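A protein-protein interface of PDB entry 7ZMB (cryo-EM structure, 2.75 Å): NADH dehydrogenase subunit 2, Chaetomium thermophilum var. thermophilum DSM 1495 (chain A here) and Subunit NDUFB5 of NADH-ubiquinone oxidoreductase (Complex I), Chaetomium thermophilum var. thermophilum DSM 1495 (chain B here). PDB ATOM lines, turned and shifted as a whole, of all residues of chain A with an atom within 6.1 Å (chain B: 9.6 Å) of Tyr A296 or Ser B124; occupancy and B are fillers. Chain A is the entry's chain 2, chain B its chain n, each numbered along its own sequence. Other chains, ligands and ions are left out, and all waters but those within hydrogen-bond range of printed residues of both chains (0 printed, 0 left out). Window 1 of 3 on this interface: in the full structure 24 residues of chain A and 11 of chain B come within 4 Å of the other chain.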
ATOM      1  N   LYS A  49       5.627  25.743 -13.843  1.00  0.00           N
ATOM      2  CA  LYS A  49       4.693  24.769 -13.246  1.00  0.00           C
ATOM      3  C   LYS A  49       3.759  25.520 -12.300  1.00  0.00           C
ATOM      4  O   LYS A  49       2.565  25.209 -12.303  1.00  0.00           O
ATOM      5  CB  LYS A  49       5.473  23.679 -12.507  1.00  0.00           C
ATOM      6  CG  LYS A  49       6.079  22.608 -13.394  1.00  0.00           C
ATOM      7  CD  LYS A  49       6.169  21.269 -12.713  1.00  0.00           C
ATOM      8  CE  LYS A  49       6.933  20.277 -13.553  1.00  0.00           C
ATOM      9  NZ  LYS A  49       8.044  20.961 -14.249  1.00  0.00           N
ATOM     10  N   LEU A 291      -8.303  18.726  -8.841  1.00  0.00           N
ATOM     11  CA  LEU A 291      -7.890  17.326  -8.579  1.00  0.00           C
ATOM     12  C   LEU A 291      -6.715  16.933  -9.480  1.00  0.00           C
ATOM     13  O   LEU A 291      -5.893  16.133  -9.030  1.00  0.00           O
ATOM     14  CB  LEU A 291      -9.096  16.389  -8.694  1.00  0.00           C
ATOM     15  CG  LEU A 291     -10.233  16.630  -7.704  1.00  0.00           C
ATOM     16  CD1 LEU A 291     -11.425  15.754  -8.044  1.00  0.00           C
ATOM     17  CD2 LEU A 291      -9.779  16.378  -6.277  1.00  0.00           C
ATOM     18  N   LEU A 292      -6.615  17.503 -10.682  1.00  0.00           N
ATOM     19  CA  LEU A 292      -5.542  17.151 -11.649  1.00  0.00           C
ATOM     20  C   LEU A 292      -4.151  17.422 -11.082  1.00  0.00           C
ATOM     21  O   LEU A 292      -3.293  16.535 -11.199  1.00  0.00           O
ATOM     22  CB  LEU A 292      -5.765  17.969 -12.923  1.00  0.00           C
ATOM     23  CG  LEU A 292      -4.675  17.868 -13.990  1.00  0.00           C
ATOM     24  CD1 LEU A 292      -4.530  16.441 -14.495  1.00  0.00           C
ATOM     25  CD2 LEU A 292      -4.965  18.808 -15.145  1.00  0.00           C
ATOM     26  N   GLU A 293      -3.944  18.588 -10.483  1.00  0.00           N
ATOM     27  CA  GLU A 293      -2.638  18.955  -9.890  1.00  0.00           C
ATOM     28  C   GLU A 293      -2.338  18.051  -8.693  1.00  0.00           C
ATOM     29  O   GLU A 293      -1.174  17.680  -8.508  1.00  0.00           O
ATOM     30  CB  GLU A 293      -2.601  20.447  -9.582  1.00  0.00           C
ATOM     31  CG  GLU A 293      -1.613  21.216 -10.437  1.00  0.00           C
ATOM     32  CD  GLU A 293      -1.381  22.640  -9.966  1.00  0.00           C
ATOM     33  OE1 GLU A 293      -1.191  23.524 -10.822  1.00  0.00           O
ATOM     34  OE2 GLU A 293      -1.381  22.859  -8.742  1.00  0.00           O
ATOM     35  N   LEU A 294      -3.364  17.752  -7.894  1.00  0.00           N
ATOM     36  CA  LEU A 294      -3.199  16.828  -6.746  1.00  0.00           C
ATOM     37  C   LEU A 294      -2.752  15.452  -7.263  1.00  0.00           C
ATOM     38  O   LEU A 294      -1.774  14.925  -6.724  1.00  0.00           O
ATOM     39  CB  LEU A 294      -4.543  16.739  -6.018  1.00  0.00           C
ATOM     40  CG  LEU A 294      -4.502  16.923  -4.504  1.00  0.00           C
ATOM     41  CD1 LEU A 294      -5.899  16.817  -3.916  1.00  0.00           C
ATOM     42  CD2 LEU A 294      -3.574  15.909  -3.858  1.00  0.00           C
ATOM     43  N   VAL A 295      -3.426  14.914  -8.285  1.00  0.00           N
ATOM     44  CA  VAL A 295      -3.090  13.559  -8.809  1.00  0.00           C
ATOM     45  C   VAL A 295      -1.667  13.535  -9.379  1.00  0.00           C
ATOM     46  O   VAL A 295      -0.949  12.563  -9.083  1.00  0.00           O
ATOM     47  CB  VAL A 295      -4.125  13.109  -9.863  1.00  0.00           C
ATOM     48  CG1 VAL A 295      -3.577  12.071 -10.825  1.00  0.00           C
ATOM     49  CG2 VAL A 295      -5.438  12.655  -9.252  1.00  0.00           C
ATOM     50  N   TYR A 296      -1.241  14.566 -10.108  1.00  0.00           N
ATOM     51  CA  TYR A 296       0.150  14.612 -10.622  1.00  0.00           C
ATOM     52  C   TYR A 296       1.193  14.663  -9.505  1.00  0.00           C
ATOM     53  O   TYR A 296       2.162  13.884  -9.575  1.00  0.00           O
ATOM     54  CB  TYR A 296       0.374  15.822 -11.528  1.00  0.00           C
ATOM     55  CG  TYR A 296       1.771  15.878 -12.092  1.00  0.00           C
ATOM     56  CD1 TYR A 296       2.116  15.132 -13.204  1.00  0.00           C
ATOM     57  CD2 TYR A 296       2.760  16.639 -11.493  1.00  0.00           C
ATOM     58  CE1 TYR A 296       3.401  15.149 -13.713  1.00  0.00           C
ATOM     59  CE2 TYR A 296       4.052  16.665 -11.988  1.00  0.00           C
ATOM     60  CZ  TYR A 296       4.373  15.917 -13.104  1.00  0.00           C
ATOM     61  OH  TYR A 296       5.639  15.940 -13.609  1.00  0.00           O
ATOM     62  N   TYR A 297       0.986  15.488  -8.477  1.00  0.00           N
ATOM     63  CA  TYR A 297       2.050  15.691  -7.456  1.00  0.00           C
ATOM     64  C   TYR A 297       2.025  14.621  -6.356  1.00  0.00           C
ATOM     65  O   TYR A 297       2.917  14.649  -5.493  1.00  0.00           O
ATOM     66  CB  TYR A 297       2.064  17.134  -6.936  1.00  0.00           C
ATOM     67  CG  TYR A 297       2.442  18.204  -7.926  1.00  0.00           C
ATOM     68  CD1 TYR A 297       3.747  18.350  -8.360  1.00  0.00           C
ATOM     69  CD2 TYR A 297       1.503  19.105  -8.394  1.00  0.00           C
ATOM     70  CE1 TYR A 297       4.105  19.342  -9.257  1.00  0.00           C
ATOM     71  CE2 TYR A 297       1.842  20.102  -9.292  1.00  0.00           C
ATOM     72  CZ  TYR A 297       3.148  20.221  -9.728  1.00  0.00           C
ATOM     73  OH  TYR A 297       3.488  21.202 -10.612  1.00  0.00           O
ATOM     74  N   THR A 298       1.048  13.717  -6.373  1.00  0.00           N
ATOM     75  CA  THR A 298       0.996  12.628  -5.367  1.00  0.00           C
ATOM     76  C   THR A 298       1.260  11.250  -5.986  1.00  0.00           C
ATOM     77  O   THR A 298       0.988  10.258  -5.299  1.00  0.00           O
ATOM     78  CB  THR A 298      -0.301  12.656  -4.550  1.00  0.00           C
ATOM     79  OG1 THR A 298      -1.413  12.545  -5.437  1.00  0.00           O
ATOM     80  CG2 THR A 298      -0.420  13.887  -3.677  1.00  0.00           C
ATOM     81  N   ASN A 299       1.739  11.182  -7.232  1.00  0.00           N
ATOM     82  CA  ASN A 299       1.928   9.855  -7.876  1.00  0.00           C
ATOM     83  C   ASN A 299       3.331   9.348  -7.571  1.00  0.00           C
ATOM     84  O   ASN A 299       4.297  10.034  -7.962  1.00  0.00           O
ATOM     85  CB  ASN A 299       1.758   9.891  -9.391  1.00  0.00           C
ATOM     86  CG  ASN A 299       0.579   9.080  -9.880  1.00  0.00           C
ATOM     87  OD1 ASN A 299      -0.117   8.454  -9.089  1.00  0.00           O
ATOM     88  ND2 ASN A 299       0.351   9.080 -11.182  1.00  0.00           N
ATOM     89  N   ASN A 301       6.340   7.527  -8.496  1.00  0.00           N
ATOM     90  CA  ASN A 301       6.861   6.940  -9.759  1.00  0.00           C
ATOM     91  C   ASN A 301       7.404   5.539  -9.470  1.00  0.00           C
ATOM     92  O   ASN A 301       7.133   4.626 -10.274  1.00  0.00           O
ATOM     93  CB  ASN A 301       7.896   7.855 -10.418  1.00  0.00           C
ATOM     94  CG  ASN A 301       7.341   9.218 -10.777  1.00  0.00           C
ATOM     95  OD1 ASN A 301       6.181   9.516 -10.500  1.00  0.00           O
ATOM     96  ND2 ASN A 301       8.162  10.052 -11.394  1.00  0.00           N
ATOM     97  N   SER A 358      -2.428   8.616 -15.020  1.00  0.00           N
ATOM     98  CA  SER A 358      -1.783   9.952 -15.033  1.00  0.00           C
ATOM     99  C   SER A 358      -0.590   9.864 -15.967  1.00  0.00           C
ATOM    100  O   SER A 358       0.438   9.302 -15.568  1.00  0.00           O
ATOM    101  CB  SER A 358      -1.445  10.463 -13.657  1.00  0.00           C
ATOM    102  OG  SER A 358      -0.980  11.804 -13.713  1.00  0.00           O
ATOM    103  N   LEU A 568       3.420  20.851 -17.231  1.00  0.00           N
ATOM    104  CA  LEU A 568       3.097  20.133 -15.971  1.00  0.00           C
ATOM    105  C   LEU A 568       4.038  18.950 -15.728  1.00  0.00           C
ATOM    106  O   LEU A 568       4.296  18.652 -14.556  1.00  0.00           O
ATOM    107  CB  LEU A 568       1.630  19.700 -16.008  1.00  0.00           C
ATOM    108  CG  LEU A 568       1.158  18.812 -14.856  1.00  0.00           C
ATOM    109  CD1 LEU A 568       0.871  19.634 -13.610  1.00  0.00           C
ATOM    110  CD2 LEU A 568      -0.069  18.013 -15.254  1.00  0.00           C
ATOM    111  N   PHE A 569       4.515  18.298 -16.785  1.00  0.00           N
ATOM    112  CA  PHE A 569       5.320  17.062 -16.650  1.00  0.00           C
ATOM    113  C   PHE A 569       6.803  17.295 -16.934  1.00  0.00           C
ATOM    114  O   PHE A 569       7.524  16.302 -16.940  1.00  0.00           O
ATOM    115  CB  PHE A 569       4.803  16.044 -17.670  1.00  0.00           C
ATOM    116  CG  PHE A 569       3.666  15.146 -17.260  1.00  0.00           C
ATOM    117  CD1 PHE A 569       2.363  15.610 -17.237  1.00  0.00           C
ATOM    118  CD2 PHE A 569       3.896  13.814 -16.964  1.00  0.00           C
ATOM    119  CE1 PHE A 569       1.319  14.770 -16.885  1.00  0.00           C
ATOM    120  CE2 PHE A 569       2.849  12.975 -16.615  1.00  0.00           C
ATOM    121  CZ  PHE A 569       1.563  13.456 -16.570  1.00  0.00           C
ATOM    122  N   SER A 570       7.246  18.535 -17.174  1.00  0.00           N
ATOM    123  CA  SER A 570       8.634  18.794 -17.537  1.00  0.00           C
ATOM    124  C   SER A 570       9.538  18.958 -16.322  1.00  0.00           C
ATOM    125  O   SER A 570       9.140  18.650 -15.194  1.00  0.00           O
ATOM    126  CB  SER A 570       8.729  20.036 -18.412  1.00  0.00           C
ATOM    127  OG  SER A 570       8.073  19.830 -19.644  1.00  0.00           O
ATOM    128  N   ALA A 571      10.754  19.447 -16.557  1.00  0.00           N
ATOM    129  CA  ALA A 571      11.766  19.630 -15.520  1.00  0.00           C
ATOM    130  C   ALA A 571      12.020  18.327 -14.773  1.00  0.00           C
ATOM    131  O   ALA A 571      11.919  17.244 -15.350  1.00  0.00           O
ATOM    132  CB  ALA A 571      11.355  20.735 -14.550  1.00  0.00           C
ATOM    133  N   ALA B 121       7.948  11.513 -22.972  1.00  0.00           N
ATOM    134  CA  ALA B 121       8.841  12.370 -22.161  1.00  0.00           C
ATOM    135  C   ALA B 121       8.754  11.966 -20.693  1.00  0.00           C
ATOM    136  O   ALA B 121       7.647  11.709 -20.212  1.00  0.00           O
ATOM    137  CB  ALA B 121       8.471  13.809 -22.342  1.00  0.00           C
ATOM    138  N   GLU B 122       9.892  11.937 -20.004  1.00  0.00           N
ATOM    139  CA  GLU B 122       9.923  11.479 -18.590  1.00  0.00           C
ATOM    140  C   GLU B 122       9.130  12.417 -17.681  1.00  0.00           C
ATOM    141  O   GLU B 122       9.199  13.640 -17.888  1.00  0.00           O
ATOM    142  CB  GLU B 122      11.367  11.391 -18.105  1.00  0.00           C
ATOM    143  CG  GLU B 122      12.234  10.493 -18.968  1.00  0.00           C
ATOM    144  CD  GLU B 122      13.645  10.280 -18.449  1.00  0.00           C
ATOM    145  OE1 GLU B 122      14.516   9.889 -19.251  1.00  0.00           O
ATOM    146  OE2 GLU B 122      13.869  10.503 -17.242  1.00  0.00           O
ATOM    147  N   ARG B 123       8.402  11.854 -16.716  1.00  0.00           N
ATOM    148  CA  ARG B 123       7.697  12.681 -15.706  1.00  0.00           C
ATOM    149  C   ARG B 123       8.749  13.048 -14.668  1.00  0.00           C
ATOM    150  O   ARG B 123       9.551  12.164 -14.315  1.00  0.00           O
ATOM    151  CB  ARG B 123       6.622  11.836 -15.020  1.00  0.00           C
ATOM    152  CG  ARG B 123       5.834  12.509 -13.911  1.00  0.00           C
ATOM    153  CD  ARG B 123       5.075  11.406 -13.206  1.00  0.00           C
ATOM    154  NE  ARG B 123       3.917  11.852 -12.451  1.00  0.00           N
ATOM    155  CZ  ARG B 123       2.665  11.581 -12.790  1.00  0.00           C
ATOM    156  NH1 ARG B 123       2.413  10.855 -13.863  1.00  0.00           N
ATOM    157  NH2 ARG B 123       1.672  12.028 -12.047  1.00  0.00           N
ATOM    158  N   SER B 124       8.741  14.295 -14.201  1.00  0.00           N
ATOM    159  CA  SER B 124       9.683  14.694 -13.136  1.00  0.00           C
ATOM    160  C   SER B 124       9.184  14.255 -11.770  1.00  0.00           C
ATOM    161  O   SER B 124       7.987  14.399 -11.517  1.00  0.00           O
ATOM    162  CB  SER B 124       9.921  16.162 -13.128  1.00  0.00           C
ATOM    163  OG  SER B 124      10.823  16.517 -12.093  1.00  0.00           O
ATOM    164  N   ARG B 125      10.069  13.695 -10.952  1.00  0.00           N
ATOM    165  CA  ARG B 125       9.673  13.420  -9.554  1.00  0.00           C
ATOM    166  C   ARG B 125      10.186  14.561  -8.663  1.00  0.00           C
ATOM    167  O   ARG B 125       9.708  14.662  -7.531  1.00  0.00           O
ATOM    168  CB  ARG B 125      10.130  12.023  -9.117  1.00  0.00           C
ATOM    169  CG  ARG B 125      11.633  11.796  -9.176  1.00  0.00           C
ATOM    170  CD  ARG B 125      11.960  10.356  -8.828  1.00  0.00           C
ATOM    171  NE  ARG B 125      11.497   9.427  -9.848  1.00  0.00           N
ATOM    172  CZ  ARG B 125      11.556   8.105  -9.743  1.00  0.00           C
ATOM    173  NH1 ARG B 125      12.053   7.550  -8.651  1.00  0.00           N
ATOM    174  NH2 ARG B 125      11.112   7.343 -10.726  1.00  0.00           N
ATOM    175  N   HIS B 126      11.075  15.427  -9.159  1.00  0.00           N
ATOM    176  CA  HIS B 126      11.602  16.570  -8.359  1.00  0.00           C
ATOM    177  C   HIS B 126      10.551  17.680  -8.203  1.00  0.00           C
ATOM    178  O   HIS B 126      10.075  18.175  -9.240  1.00  0.00           O
ATOM    179  CB  HIS B 126      12.943  17.064  -8.929  1.00  0.00           C
ATOM    180  CG  HIS B 126      13.369  18.425  -8.488  1.00  0.00           C
ATOM    181  ND1 HIS B 126      13.572  18.749  -7.165  1.00  0.00           N
ATOM    182  CD2 HIS B 126      13.665  19.535  -9.197  1.00  0.00           C
ATOM    183  CE1 HIS B 126      13.962  20.003  -7.074  1.00  0.00           C
ATOM    184  NE2 HIS B 126      14.024  20.507  -8.306  1.00  0.00           N
ATOM    185  N   ILE B 127      10.220  18.065  -6.959  1.00  0.00           N
ATOM    186  CA  ILE B 127       9.261  19.177  -6.726  1.00  0.00           C
ATOM    187  C   ILE B 127      10.076  20.457  -6.521  1.00  0.00           C
ATOM    188  O   ILE B 127      10.950  20.465  -5.656  1.00  0.00           O
ATOM    189  CB  ILE B 127       8.385  18.849  -5.499  1.00  0.00           C
ATOM    190  CG1 ILE B 127       7.710  17.480  -5.614  1.00  0.00           C
ATOM    191  CG2 ILE B 127       7.378  19.957  -5.234  1.00  0.00           C
ATOM    192  CD1 ILE B 127       6.514  17.463  -6.533  1.00  0.00           C
ATOM    193  N   GLU B 128       9.764  21.509  -7.278  1.00  0.00           N
ATOM    194  CA  GLU B 128      10.434  22.827  -7.123  1.00  0.00           C
ATOM    195  C   GLU B 128       9.391  23.726  -6.480  1.00  0.00           C
ATOM    196  O   GLU B 128       8.279  23.761  -7.010  1.00  0.00           O
ATOM    197  CB  GLU B 128      10.835  23.394  -8.486  1.00  0.00           C
ATOM    198  CG  GLU B 128      12.135  24.169  -8.470  1.00  0.00           C
ATOM    199  CD  GLU B 128      12.911  24.138  -9.774  1.00  0.00           C
ATOM    200  OE1 GLU B 128      12.895  23.088 -10.445  1.00  0.00           O
ATOM    201  OE2 GLU B 128      13.530  25.164 -10.117  1.00  0.00           O
ATOM    202  N   LYS B 130       6.770  26.349  -5.603  1.00  0.00           N
ATOM    203  CA  LYS B 130       6.054  27.495  -6.214  1.00  0.00           C
ATOM    204  C   LYS B 130       6.364  28.716  -5.371  1.00  0.00           C
ATOM    205  O   LYS B 130       6.470  29.812  -5.925  1.00  0.00           O
ATOM    206  CB  LYS B 130       4.549  27.237  -6.196  1.00  0.00           C
ATOM    207  CG  LYS B 130       4.034  26.174  -7.151  1.00  0.00           C
ATOM    208  CD  LYS B 130       2.601  25.796  -6.866  1.00  0.00           C
ATOM    209  CE  LYS B 130       1.948  25.043  -8.001  1.00  0.00           C
ATOM    210  NZ  LYS B 130       0.700  24.381  -7.567  1.00  0.00           N
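The backbone carbonyl oxygen of Leu A568 sits close to the side-chain hydroxyl of Tyr A296 (3.2 Å).
OG of Ser B124 lies within hydrogen-bond range of N of His B126 (3.1 Å).
NZ of Lys A49 is in hydrogen-bond range of O of Ser A570 (2.7 Å).
OD1 of Asn A301 lies close to O of Asn A299.
Of the printed residues of chain B, Tyr A296 touches Arg B123 (3.1 Å) and Ser B124 (3.5 Å).
Ser B124 touches four residues of chain A.
Tyr A297 touches one residue of chain B.
Ala A571 touches just one residue of chain B: Ser B124.
Of the printed residues of chain A, Ile B127 touches Tyr A297 (3.4 Å).
Of the printed residues of chain A, Arg B125 touches Asn A301.
Glu B128 touches none of the printed residues of chain A.
The nearest residue of chain A that does not touch Ser B124 is Asn A301 (4.3 Å).
OE2 of Glu A293 lies within salt-bridge range of NZ of Lys B130 (2.8 Å).
The backbone carbonyl oxygen (O) of Tyr A296 is in hydrogen-bond range of the guanidinium group (NH2) of Arg B123, 3.1 Å away.
The backbone carbonyl oxygen of Ser A358 lies within hydrogen-bond range of the guanidinium group of Arg B123 (3.0 Å).
O of Glu B122 lies close to O of Phe A569 (3.3 Å).
ND2 of Asn A299 sits close to NH2 of Arg B123 (3.3 Å).
Hydrophobic or aromatic side chains of chain A that line the printed part of chain B: Tyr A296, Tyr A297 and Phe A569.
Among the printed residues, 14 pairs touch across the chains.
Among the printed residues, Asp or Glu carboxylates within 4 Å of a Lys or Arg side-chain nitrogen of the other chain: Glu A293 with Lys B130 (2.8 Å).
Among the printed residues, merely in contact across the chains: Ala A571 with Ser B124 (3.2 Å), Asn A301 with Arg B125 (3.3 Å), Ser A570 with Ser B124 (3.3 Å), Tyr A297 with Ile B127 (3.4 Å), Asn A301 with Arg B123 (3.5 Å), Phe A569 with Arg B123 (3.5 Å), Tyr A296 with Ser B124 (3.5 Å), Phe A569 with Ser B124 (3.6 Å) and Val A295 with Arg B123 (3.99 Å).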
